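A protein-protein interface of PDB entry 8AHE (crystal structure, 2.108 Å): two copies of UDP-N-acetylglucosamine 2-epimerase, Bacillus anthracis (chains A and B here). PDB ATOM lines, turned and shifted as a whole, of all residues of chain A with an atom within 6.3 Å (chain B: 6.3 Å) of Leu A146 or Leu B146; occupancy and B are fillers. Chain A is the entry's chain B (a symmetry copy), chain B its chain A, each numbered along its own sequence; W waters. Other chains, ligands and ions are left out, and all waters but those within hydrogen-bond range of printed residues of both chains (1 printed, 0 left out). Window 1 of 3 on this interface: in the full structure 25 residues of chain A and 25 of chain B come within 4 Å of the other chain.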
ATOM      1  N   PHE A 109      22.493  25.195  -2.784  1.00  0.00           N
ATOM      2  CA  PHE A 109      23.536  24.173  -2.708  1.00  0.00           C
ATOM      3  C   PHE A 109      23.531  23.327  -3.992  1.00  0.00           C
ATOM      4  O   PHE A 109      24.563  23.180  -4.608  1.00  0.00           O
ATOM      5  CB  PHE A 109      23.367  23.313  -1.450  1.00  0.00           C
ATOM      6  CG  PHE A 109      24.019  21.957  -1.497  1.00  0.00           C
ATOM      7  CD1 PHE A 109      25.344  21.823  -1.851  1.00  0.00           C
ATOM      8  CD2 PHE A 109      23.288  20.821  -1.187  1.00  0.00           C
ATOM      9  CE1 PHE A 109      25.929  20.572  -1.889  1.00  0.00           C
ATOM     10  CE2 PHE A 109      23.876  19.575  -1.238  1.00  0.00           C
ATOM     11  CZ  PHE A 109      25.183  19.446  -1.616  1.00  0.00           C
ATOM     12  N   SER A 112      24.500  25.227  -7.193  1.00  0.00           N
ATOM     13  CA  SER A 112      25.942  25.340  -7.235  1.00  0.00           C
ATOM     14  C   SER A 112      26.558  24.009  -7.662  1.00  0.00           C
ATOM     15  O   SER A 112      27.464  23.991  -8.504  1.00  0.00           O
ATOM     16  CB  SER A 112      26.520  25.831  -5.891  1.00  0.00           C
ATOM     17  OG  SER A 112      25.834  26.980  -5.394  1.00  0.00           O
ATOM     18  N   LEU A 113      26.087  22.887  -7.120  1.00  0.00           N
ATOM     19  CA  LEU A 113      26.688  21.618  -7.468  1.00  0.00           C
ATOM     20  C   LEU A 113      26.460  21.326  -8.961  1.00  0.00           C
ATOM     21  O   LEU A 113      27.321  20.776  -9.620  1.00  0.00           O
ATOM     22  CB  LEU A 113      26.090  20.512  -6.577  1.00  0.00           C
ATOM     23  CG  LEU A 113      26.729  19.121  -6.779  1.00  0.00           C
ATOM     24  CD1 LEU A 113      28.198  19.156  -6.374  1.00  0.00           C
ATOM     25  CD2 LEU A 113      25.998  18.089  -5.965  1.00  0.00           C
ATOM     26  N   PHE A 116      28.903  23.334 -10.935  1.00  0.00           N
ATOM     27  CA  PHE A 116      30.207  22.719 -10.800  1.00  0.00           C
ATOM     28  C   PHE A 116      30.331  21.497 -11.712  1.00  0.00           C
ATOM     29  O   PHE A 116      31.404  21.231 -12.283  1.00  0.00           O
ATOM     30  CB  PHE A 116      30.429  22.325  -9.336  1.00  0.00           C
ATOM     31  CG  PHE A 116      31.753  21.690  -9.109  1.00  0.00           C
ATOM     32  CD1 PHE A 116      32.899  22.385  -9.410  1.00  0.00           C
ATOM     33  CD2 PHE A 116      31.822  20.350  -8.785  1.00  0.00           C
ATOM     34  CE1 PHE A 116      34.118  21.748  -9.344  1.00  0.00           C
ATOM     35  CE2 PHE A 116      33.045  19.733  -8.671  1.00  0.00           C
ATOM     36  CZ  PHE A 116      34.181  20.438  -8.953  1.00  0.00           C
ATOM     37  N   GLU A 141      23.122  26.013   7.741  1.00  0.00           N
ATOM     38  CA  GLU A 141      24.511  26.331   8.015  1.00  0.00           C
ATOM     39  C   GLU A 141      25.407  25.519   7.074  1.00  0.00           C
ATOM     40  O   GLU A 141      26.311  26.057   6.457  1.00  0.00           O
ATOM     41  CB  GLU A 141      24.885  26.120   9.479  1.00  0.00           C
ATOM     42  CG  GLU A 141      26.373  26.378   9.816  1.00  0.00           C
ATOM     43  CD  GLU A 141      26.870  27.821   9.774  1.00  0.00           C
ATOM     44  OE1 GLU A 141      26.038  28.751   9.657  1.00  0.00           O
ATOM     45  OE2 GLU A 141      28.098  28.009   9.914  1.00  0.00           O
ATOM     46  N   MET A 142      25.142  24.226   6.948  1.00  0.00           N
ATOM     47  CA  MET A 142      25.938  23.361   6.094  1.00  0.00           C
ATOM     48  C   MET A 142      25.772  23.745   4.626  1.00  0.00           C
ATOM     49  O   MET A 142      26.745  23.705   3.882  1.00  0.00           O
ATOM     50  CB  MET A 142      25.530  21.904   6.317  1.00  0.00           C
ATOM     51  CG  MET A 142      26.505  20.936   5.645  1.00  0.00           C
ATOM     52  SD  MET A 142      28.217  21.196   6.137  1.00  0.00           S
ATOM     53  CE  MET A 142      28.184  21.019   7.894  1.00  0.00           C
ATOM     54  N   ASN A 143      24.554  24.141   4.219  1.00  0.00           N
ATOM     55  CA  ASN A 143      24.263  24.585   2.862  1.00  0.00           C
ATOM     56  C   ASN A 143      25.164  25.769   2.523  1.00  0.00           C
ATOM     57  O   ASN A 143      25.757  25.767   1.444  1.00  0.00           O
ATOM     58  CB  ASN A 143      22.795  24.978   2.643  1.00  0.00           C
ATOM     59  CG  ASN A 143      21.855  23.803   2.594  1.00  0.00           C
ATOM     60  OD1 ASN A 143      22.243  22.653   2.299  1.00  0.00           O
ATOM     61  ND2 ASN A 143      20.594  24.106   2.869  1.00  0.00           N
ATOM     62  N   ARG A 144      25.272  26.747   3.423  1.00  0.00           N
ATOM     63  CA  ARG A 144      26.045  27.936   3.098  1.00  0.00           C
ATOM     64  C   ARG A 144      27.536  27.645   3.083  1.00  0.00           C
ATOM     65  O   ARG A 144      28.254  28.259   2.283  1.00  0.00           O
ATOM     66  CB  ARG A 144      25.516  29.183   3.836  1.00  0.00           C
ATOM     67  CG  ARG A 144      25.503  29.154   5.334  1.00  0.00           C
ATOM     68  CD  ARG A 144      24.684  30.312   5.881  1.00  0.00           C
ATOM     69  NE  ARG A 144      24.697  30.098   7.338  1.00  0.00           N
ATOM     70  CZ  ARG A 144      23.639  30.260   8.152  1.00  0.00           C
ATOM     71  NH1 ARG A 144      22.489  30.755   7.714  1.00  0.00           N
ATOM     72  NH2 ARG A 144      23.769  29.971   9.424  1.00  0.00           N
ATOM     73  N   GLN A 145      27.991  26.631   3.841  1.00  0.00           N
ATOM     74  CA  GLN A 145      29.385  26.172   3.782  1.00  0.00           C
ATOM     75  C   GLN A 145      29.716  25.423   2.482  1.00  0.00           C
ATOM     76  O   GLN A 145      30.748  25.728   1.868  1.00  0.00           O
ATOM     77  CB  GLN A 145      29.697  25.283   4.974  1.00  0.00           C
ATOM     78  CG  GLN A 145      29.438  26.003   6.283  1.00  0.00           C
ATOM     79  CD  GLN A 145      30.674  26.349   7.071  1.00  0.00           C
ATOM     80  OE1 GLN A 145      30.722  26.088   8.276  1.00  0.00           O
ATOM     81  NE2 GLN A 145      31.626  26.989   6.400  1.00  0.00           N
ATOM     82  N   LEU A 146      28.841  24.465   2.098  1.00  0.00           N
ATOM     83  CA  LEU A 146      28.923  23.703   0.869  1.00  0.00           C
ATOM     84  C   LEU A 146      28.936  24.628  -0.346  1.00  0.00           C
ATOM     85  O   LEU A 146      29.819  24.532  -1.185  1.00  0.00           O
ATOM     86  CB  LEU A 146      27.760  22.711   0.806  1.00  0.00           C
ATOM     87  CG  LEU A 146      27.837  21.533   1.791  1.00  0.00           C
ATOM     88  CD1 LEU A 146      26.511  20.796   1.792  1.00  0.00           C
ATOM     89  CD2 LEU A 146      28.978  20.551   1.472  1.00  0.00           C
ATOM     90  N   THR A 147      27.998  25.563  -0.395  1.00  0.00           N
ATOM     91  CA  THR A 147      27.902  26.582  -1.439  1.00  0.00           C
ATOM     92  C   THR A 147      29.166  27.448  -1.395  1.00  0.00           C
ATOM     93  O   THR A 147      29.735  27.776  -2.410  1.00  0.00           O
ATOM     94  CB  THR A 147      26.605  27.411  -1.236  1.00  0.00           C
ATOM     95  OG1 THR A 147      25.446  26.584  -1.438  1.00  0.00           O
ATOM     96  CG2 THR A 147      26.507  28.599  -2.162  1.00  0.00           C
ATOM     97  N   GLY A 148      29.656  27.777  -0.192  1.00  0.00           N
ATOM     98  CA  GLY A 148      30.870  28.553   0.003  1.00  0.00           C
ATOM     99  C   GLY A 148      32.069  27.929  -0.699  1.00  0.00           C
ATOM    100  O   GLY A 148      32.768  28.636  -1.376  1.00  0.00           O
ATOM    101  N   VAL A 149      32.307  26.606  -0.599  1.00  0.00           N
ATOM    102  CA  VAL A 149      33.503  26.017  -1.208  1.00  0.00           C
ATOM    103  C   VAL A 149      33.390  26.020  -2.733  1.00  0.00           C
ATOM    104  O   VAL A 149      34.421  26.011  -3.396  1.00  0.00           O
ATOM    105  CB  VAL A 149      33.894  24.636  -0.657  1.00  0.00           C
ATOM    106  CG1 VAL A 149      34.290  24.742   0.803  1.00  0.00           C
ATOM    107  CG2 VAL A 149      32.819  23.606  -0.815  1.00  0.00           C
ATOM    108  N   MET A 150      32.174  26.020  -3.278  1.00  0.00           N
ATOM    109  CA  MET A 150      31.948  25.891  -4.732  1.00  0.00           C
ATOM    110  C   MET A 150      31.939  27.255  -5.423  1.00  0.00           C
ATOM    111  O   MET A 150      32.194  27.311  -6.624  1.00  0.00           O
ATOM    112  CB  MET A 150      30.622  25.168  -5.039  1.00  0.00           C
ATOM    113  CG  MET A 150      30.762  23.650  -4.797  1.00  0.00           C
ATOM    114  SD  MET A 150      29.326  22.664  -5.231  1.00  0.00           S
ATOM    115  CE  MET A 150      28.198  23.145  -3.930  1.00  0.00           C
ATOM    116  N   ALA A 151      31.668  28.338  -4.661  1.00  0.00           N
ATOM    117  CA  ALA A 151      31.455  29.666  -5.195  1.00  0.00           C
ATOM    118  C   ALA A 151      32.745  30.253  -5.770  1.00  0.00           C
ATOM    119  O   ALA A 151      33.811  30.100  -5.194  1.00  0.00           O
ATOM    120  CB  ALA A 151      30.858  30.549  -4.142  1.00  0.00           C
ATOM    121  N   PHE B 109      32.239  12.049  -1.028  1.00  0.00           N
ATOM    122  CA  PHE B 109      31.454  13.253  -0.939  1.00  0.00           C
ATOM    123  C   PHE B 109      29.997  12.905  -0.658  1.00  0.00           C
ATOM    124  O   PHE B 109      29.419  13.461   0.250  1.00  0.00           O
ATOM    125  CB  PHE B 109      31.560  14.085  -2.221  1.00  0.00           C
ATOM    126  CG  PHE B 109      30.433  15.064  -2.453  1.00  0.00           C
ATOM    127  CD1 PHE B 109      30.040  15.952  -1.448  1.00  0.00           C
ATOM    128  CD2 PHE B 109      29.750  15.079  -3.669  1.00  0.00           C
ATOM    129  CE1 PHE B 109      28.961  16.815  -1.638  1.00  0.00           C
ATOM    130  CE2 PHE B 109      28.709  15.969  -3.865  1.00  0.00           C
ATOM    131  CZ  PHE B 109      28.314  16.812  -2.839  1.00  0.00           C
ATOM    132  N   SER B 112      29.309  11.390   2.651  1.00  0.00           N
ATOM    133  CA  SER B 112      29.311  12.422   3.659  1.00  0.00           C
ATOM    134  C   SER B 112      27.998  13.205   3.692  1.00  0.00           C
ATOM    135  O   SER B 112      27.548  13.617   4.752  1.00  0.00           O
ATOM    136  CB  SER B 112      30.529  13.326   3.460  1.00  0.00           C
ATOM    137  OG  SER B 112      31.716  12.590   3.659  1.00  0.00           O
ATOM    138  N   LEU B 113      27.440  13.520   2.527  1.00  0.00           N
ATOM    139  CA  LEU B 113      26.136  14.149   2.447  1.00  0.00           C
ATOM    140  C   LEU B 113      25.024  13.258   3.015  1.00  0.00           C
ATOM    141  O   LEU B 113      24.159  13.752   3.737  1.00  0.00           O
ATOM    142  CB  LEU B 113      25.864  14.496   0.978  1.00  0.00           C
ATOM    143  CG  LEU B 113      24.717  15.459   0.728  1.00  0.00           C
ATOM    144  CD1 LEU B 113      24.891  16.747   1.524  1.00  0.00           C
ATOM    145  CD2 LEU B 113      24.627  15.742  -0.759  1.00  0.00           C
ATOM    146  N   PHE B 116      25.327  13.398   6.733  1.00  0.00           N
ATOM    147  CA  PHE B 116      24.825  14.709   7.164  1.00  0.00           C
ATOM    148  C   PHE B 116      23.282  14.777   7.146  1.00  0.00           C
ATOM    149  O   PHE B 116      22.650  15.288   8.087  1.00  0.00           O
ATOM    150  CB  PHE B 116      25.468  15.836   6.373  1.00  0.00           C
ATOM    151  CG  PHE B 116      24.858  17.176   6.710  1.00  0.00           C
ATOM    152  CD1 PHE B 116      25.065  17.767   7.941  1.00  0.00           C
ATOM    153  CD2 PHE B 116      24.039  17.840   5.801  1.00  0.00           C
ATOM    154  CE1 PHE B 116      24.417  18.958   8.259  1.00  0.00           C
ATOM    155  CE2 PHE B 116      23.455  19.070   6.102  1.00  0.00           C
ATOM    156  CZ  PHE B 116      23.611  19.613   7.349  1.00  0.00           C
ATOM    157  N   TYR B 117      22.673  14.228   6.099  1.00  0.00           N
ATOM    158  CA  TYR B 117      21.220  14.157   5.986  1.00  0.00           C
ATOM    159  C   TYR B 117      20.577  13.200   7.001  1.00  0.00           C
ATOM    160  O   TYR B 117      19.341  13.142   7.089  1.00  0.00           O
ATOM    161  CB  TYR B 117      20.805  13.796   4.548  1.00  0.00           C
ATOM    162  CG  TYR B 117      20.896  14.928   3.543  1.00  0.00           C
ATOM    163  CD1 TYR B 117      21.294  16.218   3.889  1.00  0.00           C
ATOM    164  CD2 TYR B 117      20.604  14.706   2.206  1.00  0.00           C
ATOM    165  CE1 TYR B 117      21.391  17.248   2.945  1.00  0.00           C
ATOM    166  CE2 TYR B 117      20.723  15.709   1.258  1.00  0.00           C
ATOM    167  CZ  TYR B 117      21.061  16.991   1.631  1.00  0.00           C
ATOM    168  OH  TYR B 117      21.052  17.967   0.686  1.00  0.00           O
ATOM    169  N   GLU B 141      39.431  17.795  -6.211  1.00  0.00           N
ATOM    170  CA  GLU B 141      39.692  18.940  -5.364  1.00  0.00           C
ATOM    171  C   GLU B 141      38.421  19.369  -4.629  1.00  0.00           C
ATOM    172  O   GLU B 141      38.457  19.523  -3.404  1.00  0.00           O
ATOM    173  CB  GLU B 141      40.287  20.112  -6.147  1.00  0.00           C
ATOM    174  CG  GLU B 141      40.568  21.375  -5.323  1.00  0.00           C
ATOM    175  CD  GLU B 141      41.528  21.288  -4.156  1.00  0.00           C
ATOM    176  OE1 GLU B 141      42.305  20.315  -4.085  1.00  0.00           O
ATOM    177  OE2 GLU B 141      41.488  22.205  -3.318  1.00  0.00           O
ATOM    178  N   MET B 142      37.326  19.599  -5.360  1.00  0.00           N
ATOM    179  CA  MET B 142      36.063  20.045  -4.765  1.00  0.00           C
ATOM    180  C   MET B 142      35.465  18.964  -3.845  1.00  0.00           C
ATOM    181  O   MET B 142      34.979  19.288  -2.765  1.00  0.00           O
ATOM    182  CB  MET B 142      35.051  20.417  -5.848  1.00  0.00           C
ATOM    183  CG  MET B 142      33.860  21.188  -5.349  1.00  0.00           C
ATOM    184  SD  MET B 142      34.386  22.731  -4.562  1.00  0.00           S
ATOM    185  CE  MET B 142      35.113  23.616  -5.885  1.00  0.00           C
ATOM    186  N   ASN B 143      35.544  17.674  -4.225  1.00  0.00           N
ATOM    187  CA  ASN B 143      35.031  16.588  -3.416  1.00  0.00           C
ATOM    188  C   ASN B 143      35.683  16.647  -2.036  1.00  0.00           C
ATOM    189  O   ASN B 143      35.037  16.347  -1.035  1.00  0.00           O
ATOM    190  CB  ASN B 143      35.275  15.210  -4.023  1.00  0.00           C
ATOM    191  CG  ASN B 143      34.399  14.848  -5.207  1.00  0.00           C
ATOM    192  OD1 ASN B 143      33.345  15.416  -5.433  1.00  0.00           O
ATOM    193  ND2 ASN B 143      34.851  13.878  -5.984  1.00  0.00           N
ATOM    194  N   ARG B 144      36.985  16.926  -1.950  1.00  0.00           N
ATOM    195  CA  ARG B 144      37.643  16.857  -0.645  1.00  0.00           C
ATOM    196  C   ARG B 144      37.349  18.129   0.152  1.00  0.00           C
ATOM    197  O   ARG B 144      37.240  18.059   1.393  1.00  0.00           O
ATOM    198  CB  ARG B 144      39.117  16.477  -0.780  1.00  0.00           C
ATOM    199  CG  ARG B 144      40.035  17.472  -1.475  1.00  0.00           C
ATOM    200  CD  ARG B 144      41.378  16.811  -1.759  1.00  0.00           C
ATOM    201  NE  ARG B 144      42.103  17.576  -2.766  1.00  0.00           N
ATOM    202  CZ  ARG B 144      42.907  17.077  -3.695  1.00  0.00           C
ATOM    203  NH1 ARG B 144      43.066  15.773  -3.784  1.00  0.00           N
ATOM    204  NH2 ARG B 144      43.506  17.901  -4.543  1.00  0.00           N
ATOM    205  N   GLN B 145      37.134  19.253  -0.561  1.00  0.00           N
ATOM    206  CA  GLN B 145      36.653  20.481   0.063  1.00  0.00           C
ATOM    207  C   GLN B 145      35.226  20.322   0.599  1.00  0.00           C
ATOM    208  O   GLN B 145      34.977  20.674   1.752  1.00  0.00           O
ATOM    209  CB  GLN B 145      36.769  21.654  -0.905  1.00  0.00           C
ATOM    210  CG  GLN B 145      38.196  22.159  -1.022  1.00  0.00           C
ATOM    211  CD  GLN B 145      38.273  23.560  -1.573  1.00  0.00           C
ATOM    212  OE1 GLN B 145      37.614  24.452  -1.059  1.00  0.00           O
ATOM    213  NE2 GLN B 145      39.183  23.784  -2.525  1.00  0.00           N
ATOM    214  N   LEU B 146      34.320  19.720  -0.198  1.00  0.00           N
ATOM    215  CA  LEU B 146      32.948  19.408   0.202  1.00  0.00           C
ATOM    216  C   LEU B 146      32.900  18.432   1.371  1.00  0.00           C
ATOM    217  O   LEU B 146      32.244  18.672   2.396  1.00  0.00           O
ATOM    218  CB  LEU B 146      32.172  18.842  -0.988  1.00  0.00           C
ATOM    219  CG  LEU B 146      31.919  19.821  -2.127  1.00  0.00           C
ATOM    220  CD1 LEU B 146      31.504  19.102  -3.357  1.00  0.00           C
ATOM    221  CD2 LEU B 146      30.870  20.836  -1.744  1.00  0.00           C
ATOM    222  N   THR B 147      33.619  17.336   1.232  1.00  0.00           N
ATOM    223  CA  THR B 147      33.749  16.380   2.321  1.00  0.00           C
ATOM    224  C   THR B 147      34.264  17.087   3.577  1.00  0.00           C
ATOM    225  O   THR B 147      33.771  16.840   4.684  1.00  0.00           O
ATOM    226  CB  THR B 147      34.649  15.217   1.866  1.00  0.00           C
ATOM    227  OG1 THR B 147      34.016  14.558   0.778  1.00  0.00           O
ATOM    228  CG2 THR B 147      34.916  14.221   2.971  1.00  0.00           C
ATOM    229  N   GLY B 148      35.260  17.986   3.413  1.00  0.00           N
ATOM    230  CA  GLY B 148      35.873  18.701   4.530  1.00  0.00           C
ATOM    231  C   GLY B 148      34.876  19.532   5.368  1.00  0.00           C
ATOM    232  O   GLY B 148      34.986  19.515   6.600  1.00  0.00           O
ATOM    233  N   VAL B 149      33.911  20.265   4.751  1.00  0.00           N
ATOM    234  CA  VAL B 149      32.966  21.097   5.523  1.00  0.00           C
ATOM    235  C   VAL B 149      32.010  20.220   6.335  1.00  0.00           C
ATOM    236  O   VAL B 149      31.589  20.647   7.408  1.00  0.00           O
ATOM    237  CB  VAL B 149      32.200  22.175   4.705  1.00  0.00           C
ATOM    238  CG1 VAL B 149      33.159  23.291   4.254  1.00  0.00           C
ATOM    239  CG2 VAL B 149      31.480  21.636   3.507  1.00  0.00           C
ATOM    240  N   MET B 150      31.761  18.986   5.845  1.00  0.00           N
ATOM    241  CA  MET B 150      30.828  18.027   6.438  1.00  0.00           C
ATOM    242  C   MET B 150      31.480  17.131   7.480  1.00  0.00           C
ATOM    243  O   MET B 150      30.791  16.606   8.335  1.00  0.00           O
ATOM    244  CB  MET B 150      30.184  17.149   5.367  1.00  0.00           C
ATOM    245  CG  MET B 150      29.144  17.964   4.524  1.00  0.00           C
ATOM    246  SD  MET B 150      28.258  16.992   3.286  1.00  0.00           S
ATOM    247  CE  MET B 150      29.513  16.864   2.000  1.00  0.00           C
ATOM    248  N   ALA B 151      32.797  17.056   7.541  1.00  0.00           N
ATOM    249  CA  ALA B 151      33.448  16.113   8.434  1.00  0.00           C
ATOM    250  C   ALA B 151      33.509  16.639   9.870  1.00  0.00           C
ATOM    251  O   ALA B 151      33.623  17.848  10.091  1.00  0.00           O
ATOM    252  CB  ALA B 151      34.816  15.775   7.869  1.00  0.00           C
HETATM  253  O   HOH W   1      20.626  20.594   1.841  1.00  0.00           O
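The backbone NH of Leu B113 sits close to the side-chain sulfur of Met B150 (3.6 Å).
The side-chain carboxylate (OE2) of Glu B141 lies within hydrogen-bond range of the side-chain amide nitrogen (NE2) of Gln B145 (2.9 Å).
SD of Met A150 lies close to N of Leu A113 (3.8 Å).
Of the 16 printed residues of chain B, 8 touch a printed residue of chain A.
Printed residues of chain A that touch a printed residue of chain B: Phe A109, Phe A116, Met A142, Gln A145, Leu A146, Val A149 and Met A150.
Among the printed residues, 15 pairs touch across the chains.
Among the printed residues, no Asp or Glu carboxylate lies within 4 Å of a Lys or Arg side-chain nitrogen of the other chain.
Water W1 lies within hydrogen-bond range of the side-chain amide oxygen (OD1) of Asn A143 (2.7 Å) and the side-chain hydroxyl (OH) of Tyr B117 (2.9 Å).
Leu A146 touches just these residues of chain B: Leu B146 (3.7 Å), Val B149 (3.4 Å) and Met B150 (3.8 Å).
Printed residues of chain A within 4 Å of Phe B116: Met A142 (3.2 Å).
Of the printed residues of chain B, Phe A109 touches Leu B113 and Tyr B117.
Printed residues of chain B within 4 Å of Met A142: Phe B116 (3.2 Å), Val B149 (3.5 Å) and Met B150 (3.7 Å).
Printed residues of chain A within 4 Å of Val B149: Met A142, Gln A145, Leu A146 and Val A149.
The nearest printed residue of chain A that does not touch Met B150 is Phe A109 (6.2 Å).
Phe A109 touches Leu B113, but with the chains exchanged Leu A113 does not touch Phe B109 (4.03 Å).
Met A142 touches Val B149, and with the chains exchanged Val A149 touches Met B142.
Leu B146 touches its own counterpart, Leu A146.
Leu A146 touches Met B150, but with the chains exchanged Met A150 does not touch Leu B146 (4.2 Å).
15 positions are printed for both chains.
CD2 of Leu B113 touches CZ of Phe A109 (3.8 Å).
Met B142 touches Phe A116.
Met B150 touches Met A142.
Val B149 touches Gln A145.
CD2 of Leu B146 touches CD2 of Leu A146 (3.7 Å).
Leu A146 touches Val B149 (CD2 to CG2, 3.4 Å).
CE of Met B150 touches CD2 of Leu A146, 3.8 Å away.
Gln B145 touches Val A149 (OE1 to CB, 3.7 Å).
Val A149 touches Val B149 (CG1 to CG1, 3.9 Å).
CG of Met A150 touches SD of Met B142, at 3.7 Å.
The side-chain sulfur of Met A142 lies close to the backbone carbonyl oxygen of Val B149.
SD of Met B142 sits close to O of Val A149 (3.5 Å).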
